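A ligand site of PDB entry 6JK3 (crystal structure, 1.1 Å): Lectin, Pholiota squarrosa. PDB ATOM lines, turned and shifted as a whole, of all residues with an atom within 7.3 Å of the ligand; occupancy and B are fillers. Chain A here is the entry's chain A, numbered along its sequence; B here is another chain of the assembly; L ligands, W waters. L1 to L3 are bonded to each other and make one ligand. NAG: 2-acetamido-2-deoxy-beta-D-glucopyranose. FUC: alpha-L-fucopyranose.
Asp 11 touches the ligand.
O of Val 36 touches C8 of NAG L1, at 3.6 Å.
CG1 of Val 3 of chain B touches C4 of FUC L3, 3.96 Å away.
Leu 21 of chain B touches the ligand.
CZ of Phe 23 of chain B touches O5 of NAG L2, 3.4 Å away.
CH2 of Trp 28 of chain B touches C6 of NAG L2, 3.6 Å away.
Along chain A the residues within 4 Å of the ligand span positions 11 to 36.
The nearest printed residue that does not touch the ligand is Cys 10 (4.1 Å).
The side-chain carboxylate of Asp 13 lies within hydrogen-bond range of the backbone NH of Ala 1 of chain B, 3.1 Å away.
N of Ala 1 of chain B lies within hydrogen-bond range of OD1 of Asp 11 (2.8 Å).
The backbone NH (N) of Asp 13 sits at hydrogen-bond distance from the side-chain carboxylate (OD1) of Asp 11, 2.8 Å away.
The backbone NH of Leu 21 of chain B is in hydrogen-bond range of the backbone carbonyl oxygen of Trp 28 of chain B (3.0 Å).
OD1 of Asp 11 sits at hydrogen-bond distance from N of Thr 14.
N of Val 3 of chain B sits at hydrogen-bond distance from O of Cys 10 (2.8 Å).
Water W5 lies within hydrogen-bond range of O4 of NAG L1 (2.6 Å) and OD1 of Asp 13 (3.2 Å).
Water W4 lies within hydrogen-bond range of O of Asp 13 and O4 of NAG L1.
The backbone NH (N) of Ala 1 of chain B lies within hydrogen-bond range of an oxygen (O3) of FUC L3, at 2.9 Å.
The backbone carbonyl oxygen (O) of Ala 1 of chain B sits at hydrogen-bond distance from an oxygen (O4) of FUC L3, 2.7 Å away.
The side-chain carboxylate of Asp 13 lies within hydrogen-bond range of an oxygen (O2) of FUC L3 (2.8 Å).
N of Gly 12 sits at hydrogen-bond distance from O4 of FUC L3 (2.9 Å).
N2 of NAG L1 lies within hydrogen-bond range of O of Gly 12 (2.8 Å).
An oxygen (O3) of NAG L1 is in hydrogen-bond range of the side-chain hydroxyl (OH) of Tyr 15 (2.8 Å).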
ATOM      1  N   CYS A  10       0.316  29.129   7.152  1.00  0.00           N
ATOM      2  CA  CYS A  10      -0.815  28.367   7.707  1.00  0.00           C
ATOM      3  C   CYS A  10      -1.740  29.319   8.437  1.00  0.00           C
ATOM      4  O   CYS A  10      -1.291  30.387   8.883  1.00  0.00           O
ATOM      5  CB  CYS A  10      -0.355  27.246   8.619  1.00  0.00           C
ATOM      6  SG  CYS A  10       0.805  26.050   7.897  1.00  0.00           S
ATOM      7  N   ASP A  11      -2.984  28.909   8.584  1.00  0.00           N
ATOM      8  CA  ASP A  11      -4.043  29.838   9.035  1.00  0.00           C
ATOM      9  C   ASP A  11      -4.919  29.133  10.066  1.00  0.00           C
ATOM     10  O   ASP A  11      -5.570  28.126   9.711  1.00  0.00           O
ATOM     11  CB  ASP A  11      -4.810  30.267   7.801  1.00  0.00           C
ATOM     12  CG  ASP A  11      -5.860  31.318   8.028  1.00  0.00           C
ATOM     13  OD1 ASP A  11      -6.379  31.413   9.163  1.00  0.00           O
ATOM     14  OD2 ASP A  11      -6.171  32.009   7.036  1.00  0.00           O
ATOM     15  N   GLY A  12      -4.935  29.627  11.293  1.00  0.00           N
ATOM     16  CA  GLY A  12      -5.761  29.043  12.355  1.00  0.00           C
ATOM     17  C   GLY A  12      -7.204  29.504  12.353  1.00  0.00           C
ATOM     18  O   GLY A  12      -7.937  29.094  13.262  1.00  0.00           O
ATOM     19  N   ASP A  13      -7.627  30.321  11.386  1.00  0.00           N
ATOM     20  CA  ASP A  13      -9.076  30.583  11.175  1.00  0.00           C
ATOM     21  C   ASP A  13      -9.662  29.587  10.172  1.00  0.00           C
ATOM     22  O   ASP A  13     -10.788  29.113  10.380  1.00  0.00           O
ATOM     23  CB  ASP A  13      -9.296  32.018  10.755  1.00  0.00           C
ATOM     24  CG  ASP A  13      -8.965  33.017  11.831  1.00  0.00           C
ATOM     25  OD1 ASP A  13      -9.083  32.697  13.026  1.00  0.00           O
ATOM     26  OD2 ASP A  13      -8.614  34.111  11.465  1.00  0.00           O
ATOM     27  N   THR A  14      -8.937  29.299   9.107  1.00  0.00           N
ATOM     28  CA  THR A  14      -9.423  28.360   8.067  1.00  0.00           C
ATOM     29  C   THR A  14      -8.938  26.940   8.327  1.00  0.00           C
ATOM     30  O   THR A  14      -9.496  26.012   7.717  1.00  0.00           O
ATOM     31  CB  THR A  14      -8.932  28.772   6.682  1.00  0.00           C
ATOM     32  OG1 THR A  14      -7.504  28.750   6.700  1.00  0.00           O
ATOM     33  CG2 THR A  14      -9.446  30.125   6.278  1.00  0.00           C
ATOM     34  N   TYR A  15      -7.931  26.751   9.174  1.00  0.00           N
ATOM     35  CA  TYR A  15      -7.360  25.412   9.423  1.00  0.00           C
ATOM     36  C   TYR A  15      -6.843  24.838   8.102  1.00  0.00           C
ATOM     37  O   TYR A  15      -7.115  23.683   7.745  1.00  0.00           O
ATOM     38  CB  TYR A  15      -8.355  24.486  10.146  1.00  0.00           C
ATOM     39  CG  TYR A  15      -8.632  24.947  11.544  1.00  0.00           C
ATOM     40  CD1 TYR A  15      -9.631  25.875  11.798  1.00  0.00           C
ATOM     41  CD2 TYR A  15      -7.880  24.497  12.607  1.00  0.00           C
ATOM     42  CE1 TYR A  15      -9.846  26.345  13.078  1.00  0.00           C
ATOM     43  CE2 TYR A  15      -8.074  24.976  13.894  1.00  0.00           C
ATOM     44  CZ  TYR A  15      -9.079  25.891  14.129  1.00  0.00           C
ATOM     45  OH  TYR A  15      -9.290  26.330  15.405  1.00  0.00           O
ATOM     46  N   ASN A  35      -4.729  20.560  11.268  1.00  0.00           N
ATOM     47  CA  ASN A  35      -5.022  20.980  12.655  1.00  0.00           C
ATOM     48  C   ASN A  35      -4.141  22.201  12.949  1.00  0.00           C
ATOM     49  O   ASN A  35      -3.041  22.316  12.373  1.00  0.00           O
ATOM     50  CB  ASN A  35      -4.754  19.845  13.625  1.00  0.00           C
ATOM     51  CG  ASN A  35      -5.584  18.618  13.315  1.00  0.00           C
ATOM     52  OD1 ASN A  35      -5.032  17.584  12.933  1.00  0.00           O
ATOM     53  ND2 ASN A  35      -6.885  18.755  13.419  1.00  0.00           N
ATOM     54  N   VAL A  36      -4.621  23.123  13.774  1.00  0.00           N
ATOM     55  CA  VAL A  36      -3.838  24.283  14.233  1.00  0.00           C
ATOM     56  C   VAL A  36      -4.100  24.408  15.714  1.00  0.00           C
ATOM     57  O   VAL A  36      -5.250  24.436  16.101  1.00  0.00           O
ATOM     58  CB  VAL A  36      -4.183  25.575  13.479  1.00  0.00           C
ATOM     59  CG1 VAL A  36      -3.308  26.715  14.006  1.00  0.00           C
ATOM     60  CG2 VAL A  36      -3.996  25.395  11.986  1.00  0.00           C
ATOM     61  N   PHE A  37      -3.057  24.434  16.520  1.00  0.00           N
ATOM     62  CA  PHE A  37      -3.249  24.440  17.986  1.00  0.00           C
ATOM     63  C   PHE A  37      -2.018  24.991  18.684  1.00  0.00           C
ATOM     64  O   PHE A  37      -0.939  25.118  18.112  1.00  0.00           O
ATOM     65  CB  PHE A  37      -3.617  23.040  18.486  1.00  0.00           C
ATOM     66  CG  PHE A  37      -2.618  21.951  18.160  1.00  0.00           C
ATOM     67  CD1 PHE A  37      -1.546  21.686  19.008  1.00  0.00           C
ATOM     68  CD2 PHE A  37      -2.776  21.172  17.030  1.00  0.00           C
ATOM     69  CE1 PHE A  37      -0.663  20.681  18.697  1.00  0.00           C
ATOM     70  CE2 PHE A  37      -1.881  20.157  16.736  1.00  0.00           C
ATOM     71  CZ  PHE A  37      -0.826  19.921  17.558  1.00  0.00           C
ATOM     72  N   HIS A  38      -2.244  25.307  19.941  1.00  0.00           N
ATOM     73  CA  HIS A  38      -1.248  25.895  20.838  1.00  0.00           C
ATOM     74  C   HIS A  38      -0.593  24.784  21.649  1.00  0.00           C
ATOM     75  O   HIS A  38      -1.267  23.899  22.148  1.00  0.00           O
ATOM     76  CB  HIS A  38      -1.939  26.927  21.732  1.00  0.00           C
ATOM     77  CG  HIS A  38      -1.000  27.672  22.618  1.00  0.00           C
ATOM     78  ND1 HIS A  38      -0.842  27.373  23.945  1.00  0.00           N
ATOM     79  CD2 HIS A  38      -0.172  28.695  22.362  1.00  0.00           C
ATOM     80  CE1 HIS A  38       0.047  28.168  24.477  1.00  0.00           C
ATOM     81  NE2 HIS A  38       0.436  29.034  23.551  1.00  0.00           N
ATOM     82  N   ALA B   1      -5.950  34.137   9.861  1.00  0.00           N
ATOM     83  CA  ALA B   1      -5.190  34.731   8.750  1.00  0.00           C
ATOM     84  C   ALA B   1      -3.925  33.920   8.578  1.00  0.00           C
ATOM     85  O   ALA B   1      -3.407  33.356   9.532  1.00  0.00           O
ATOM     86  CB  ALA B   1      -4.847  36.164   9.046  1.00  0.00           C
ATOM     87  N   PRO B   2      -3.370  33.913   7.369  1.00  0.00           N
ATOM     88  CA  PRO B   2      -2.154  33.139   7.131  1.00  0.00           C
ATOM     89  C   PRO B   2      -0.958  33.774   7.830  1.00  0.00           C
ATOM     90  O   PRO B   2      -0.750  34.956   7.727  1.00  0.00           O
ATOM     91  CB  PRO B   2      -1.989  33.181   5.621  1.00  0.00           C
ATOM     92  CG  PRO B   2      -2.741  34.382   5.191  1.00  0.00           C
ATOM     93  CD  PRO B   2      -3.898  34.494   6.147  1.00  0.00           C
ATOM     94  N   VAL B   3      -0.169  32.937   8.513  1.00  0.00           N
ATOM     95  CA  VAL B   3       1.060  33.366   9.206  1.00  0.00           C
ATOM     96  C   VAL B   3       2.213  32.503   8.711  1.00  0.00           C
ATOM     97  O   VAL B   3       2.027  31.385   8.227  1.00  0.00           O
ATOM     98  CB  VAL B   3       0.912  33.284  10.731  1.00  0.00           C
ATOM     99  CG1 VAL B   3      -0.171  34.219  11.215  1.00  0.00           C
ATOM    100  CG2 VAL B   3       0.651  31.861  11.206  1.00  0.00           C
ATOM    101  N   LEU B  21       4.736  27.855  13.769  1.00  0.00           N
ATOM    102  CA  LEU B  21       4.191  29.111  13.212  1.00  0.00           C
ATOM    103  C   LEU B  21       4.788  30.329  13.907  1.00  0.00           C
ATOM    104  O   LEU B  21       5.043  30.311  15.124  1.00  0.00           O
ATOM    105  CB  LEU B  21       2.679  29.151  13.356  1.00  0.00           C
ATOM    106  CG  LEU B  21       1.947  27.949  12.763  1.00  0.00           C
ATOM    107  CD1 LEU B  21       0.446  28.120  12.905  1.00  0.00           C
ATOM    108  CD2 LEU B  21       2.346  27.692  11.305  1.00  0.00           C
ATOM    109  N   ASP B  22       4.951  31.401  13.150  1.00  0.00           N
ATOM    110  CA  ASP B  22       5.347  32.710  13.696  1.00  0.00           C
ATOM    111  C   ASP B  22       4.072  33.459  14.011  1.00  0.00           C
ATOM    112  O   ASP B  22       3.452  34.039  13.105  1.00  0.00           O
ATOM    113  CB  ASP B  22       6.236  33.451  12.718  1.00  0.00           C
ATOM    114  CG  ASP B  22       6.627  34.826  13.225  1.00  0.00           C
ATOM    115  OD1 ASP B  22       6.439  35.099  14.411  1.00  0.00           O
ATOM    116  OD2 ASP B  22       7.064  35.632  12.418  1.00  0.00           O
ATOM    117  N   PHE B  23       3.675  33.459  15.284  1.00  0.00           N
ATOM    118  CA  PHE B  23       2.391  34.063  15.719  1.00  0.00           C
ATOM    119  C   PHE B  23       2.344  34.071  17.231  1.00  0.00           C
ATOM    120  O   PHE B  23       2.717  33.065  17.870  1.00  0.00           O
ATOM    121  CB  PHE B  23       1.198  33.263  15.157  1.00  0.00           C
ATOM    122  CG  PHE B  23      -0.116  33.723  15.717  1.00  0.00           C
ATOM    123  CD1 PHE B  23      -0.718  34.860  15.215  1.00  0.00           C
ATOM    124  CD2 PHE B  23      -0.698  33.088  16.797  1.00  0.00           C
ATOM    125  CE1 PHE B  23      -1.875  35.349  15.797  1.00  0.00           C
ATOM    126  CE2 PHE B  23      -1.876  33.566  17.358  1.00  0.00           C
ATOM    127  CZ  PHE B  23      -2.449  34.700  16.858  1.00  0.00           C
ATOM    128  N   GLY B  24       1.829  35.156  17.802  1.00  0.00           N
ATOM    129  CA  GLY B  24       1.463  35.161  19.219  1.00  0.00           C
ATOM    130  C   GLY B  24       2.656  34.848  20.098  1.00  0.00           C
ATOM    131  O   GLY B  24       3.741  35.463  19.932  1.00  0.00           O
ATOM    132  N   ASP B  25       2.490  33.910  21.022  1.00  0.00           N
ATOM    133  CA  ASP B  25       3.567  33.578  21.987  1.00  0.00           C
ATOM    134  C   ASP B  25       4.586  32.602  21.375  1.00  0.00           C
ATOM    135  O   ASP B  25       5.467  32.147  22.106  1.00  0.00           O
ATOM    136  CB  ASP B  25       2.990  32.969  23.272  1.00  0.00           C
ATOM    137  CG  ASP B  25       2.363  31.600  23.110  1.00  0.00           C
ATOM    138  OD1 ASP B  25       2.304  31.073  21.976  1.00  0.00           O
ATOM    139  OD2 ASP B  25       1.888  31.100  24.145  1.00  0.00           O
ATOM    140  N   TRP B  28       2.365  28.146  18.659  1.00  0.00           N
ATOM    141  CA  TRP B  28       1.325  27.565  17.786  1.00  0.00           C
ATOM    142  C   TRP B  28       1.976  26.725  16.705  1.00  0.00           C
ATOM    143  O   TRP B  28       3.022  27.082  16.163  1.00  0.00           O
ATOM    144  CB  TRP B  28       0.472  28.662  17.184  1.00  0.00           C
ATOM    145  CG  TRP B  28      -0.287  29.445  18.214  1.00  0.00           C
ATOM    146  CD1 TRP B  28       0.167  30.484  18.987  1.00  0.00           C
ATOM    147  CD2 TRP B  28      -1.670  29.277  18.561  1.00  0.00           C
ATOM    148  NE1 TRP B  28      -0.837  30.929  19.809  1.00  0.00           N
ATOM    149  CE2 TRP B  28      -1.972  30.215  19.562  1.00  0.00           C
ATOM    150  CE3 TRP B  28      -2.660  28.368  18.173  1.00  0.00           C
ATOM    151  CZ2 TRP B  28      -3.221  30.288  20.151  1.00  0.00           C
ATOM    152  CZ3 TRP B  28      -3.906  28.459  18.746  1.00  0.00           C
ATOM    153  CH2 TRP B  28      -4.184  29.403  19.726  1.00  0.00           C
ATOM    154  N   VAL B  29       1.278  25.660  16.339  1.00  0.00           N
ATOM    155  CA  VAL B  29       1.691  24.760  15.241  1.00  0.00           C
ATOM    156  C   VAL B  29       0.498  24.464  14.353  1.00  0.00           C
ATOM    157  O   VAL B  29      -0.649  24.510  14.804  1.00  0.00           O
ATOM    158  CB  VAL B  29       2.313  23.449  15.747  1.00  0.00           C
ATOM    159  CG1 VAL B  29       3.524  23.703  16.635  1.00  0.00           C
ATOM    160  CG2 VAL B  29       1.307  22.543  16.453  1.00  0.00           C
ATOM    161  N   ALA B  30       0.799  24.123  13.113  1.00  0.00           N
ATOM    162  CA  ALA B  30      -0.140  23.459  12.223  1.00  0.00           C
ATOM    163  C   ALA B  30       0.363  22.028  12.021  1.00  0.00           C
ATOM    164  O   ALA B  30       1.583  21.802  12.031  1.00  0.00           O
ATOM    165  CB  ALA B  30      -0.241  24.177  10.894  1.00  0.00           C
HETATM  166  C1  NAG L   1      -8.968  31.554  16.798  1.00  0.00           C
HETATM  167  C2  NAG L   1      -9.332  30.100  16.561  1.00  0.00           C
HETATM  168  C3  NAG L   1     -10.490  29.961  15.583  1.00  0.00           C
HETATM  169  C4  NAG L   1     -11.631  30.881  15.985  1.00  0.00           C
HETATM  170  C5  NAG L   1     -11.122  32.305  16.166  1.00  0.00           C
HETATM  171  C6  NAG L   1     -12.293  33.207  16.569  1.00  0.00           C
HETATM  172  C7  NAG L   1      -7.441  28.535  16.812  1.00  0.00           C
HETATM  173  C8  NAG L   1      -6.368  27.821  16.076  1.00  0.00           C
HETATM  174  N2  NAG L   1      -8.198  29.328  16.052  1.00  0.00           N
HETATM  175  O3  NAG L   1     -10.959  28.619  15.509  1.00  0.00           O
HETATM  176  O4  NAG L   1     -12.644  30.849  14.996  1.00  0.00           O
HETATM  177  O5  NAG L   1     -10.107  32.288  17.169  1.00  0.00           O
HETATM  178  O6  NAG L   1     -11.744  34.505  16.827  1.00  0.00           O
HETATM  179  O7  NAG L   1      -7.592  28.432  18.024  1.00  0.00           O
HETATM  180  C1  NAG L   2      -5.495  34.167  19.812  1.00  0.00           C
HETATM  181  C2  NAG L   2      -6.908  34.700  19.610  1.00  0.00           C
HETATM  182  C3  NAG L   2      -7.832  33.542  19.297  1.00  0.00           C
HETATM  183  C4  NAG L   2      -7.325  32.779  18.073  1.00  0.00           C
HETATM  184  C5  NAG L   2      -5.881  32.387  18.294  1.00  0.00           C
HETATM  185  C6  NAG L   2      -5.248  31.669  17.131  1.00  0.00           C
HETATM  186  C7  NAG L   2      -7.521  36.717  20.890  1.00  0.00           C
HETATM  187  C8  NAG L   2      -7.932  37.282  22.213  1.00  0.00           C
HETATM  188  N2  NAG L   2      -7.340  35.394  20.813  1.00  0.00           N
HETATM  189  O1  NAG L   2      -4.552  35.198  20.022  1.00  0.00           O
HETATM  190  O3  NAG L   2      -9.134  34.058  19.041  1.00  0.00           O
HETATM  191  O4  NAG L   2      -8.065  31.568  17.881  1.00  0.00           O
HETATM  192  O5  NAG L   2      -5.101  33.538  18.611  1.00  0.00           O
HETATM  193  O6  NAG L   2      -5.316  32.584  16.013  1.00  0.00           O
HETATM  194  O7  NAG L   2      -7.383  37.439  19.922  1.00  0.00           O
HETATM  195  C1  FUC L   3      -5.532  31.915  14.756  1.00  0.00           C
HETATM  196  C2  FUC L   3      -5.699  32.968  13.691  1.00  0.00           C
HETATM  197  C3  FUC L   3      -4.411  33.750  13.474  1.00  0.00           C
HETATM  198  C4  FUC L   3      -3.292  32.752  13.160  1.00  0.00           C
HETATM  199  C5  FUC L   3      -3.176  31.741  14.280  1.00  0.00           C
HETATM  200  C6  FUC L   3      -2.137  30.643  14.066  1.00  0.00           C
HETATM  201  O2  FUC L   3      -6.756  33.858  14.075  1.00  0.00           O
HETATM  202  O3  FUC L   3      -4.591  34.639  12.387  1.00  0.00           O
HETATM  203  O4  FUC L   3      -3.519  32.067  11.926  1.00  0.00           O
HETATM  204  O5  FUC L   3      -4.416  31.061  14.450  1.00  0.00           O
HETATM  205  O   HOH W   1     -15.102  30.720  16.100  1.00  0.00           O
HETATM  206  O   HOH W   2     -10.674  31.234  20.347  1.00  0.00           O
HETATM  207  O   HOH W   3      -1.859  34.856  21.069  1.00  0.00           O
HETATM  208  O   HOH W   4     -12.398  29.057  12.519  1.00  0.00           O
HETATM  209  O   HOH W   5     -12.203  32.101  12.704  1.00  0.00           O
HETATM  210  O   HOH W   6      -8.397  29.636  20.389  1.00  0.00           O
HETATM  211  O   HOH W   7      -5.970  35.631  16.226  1.00  0.00           O
HETATM  212  O   HOH W   8      -7.048  26.183  19.433  1.00  0.00           O
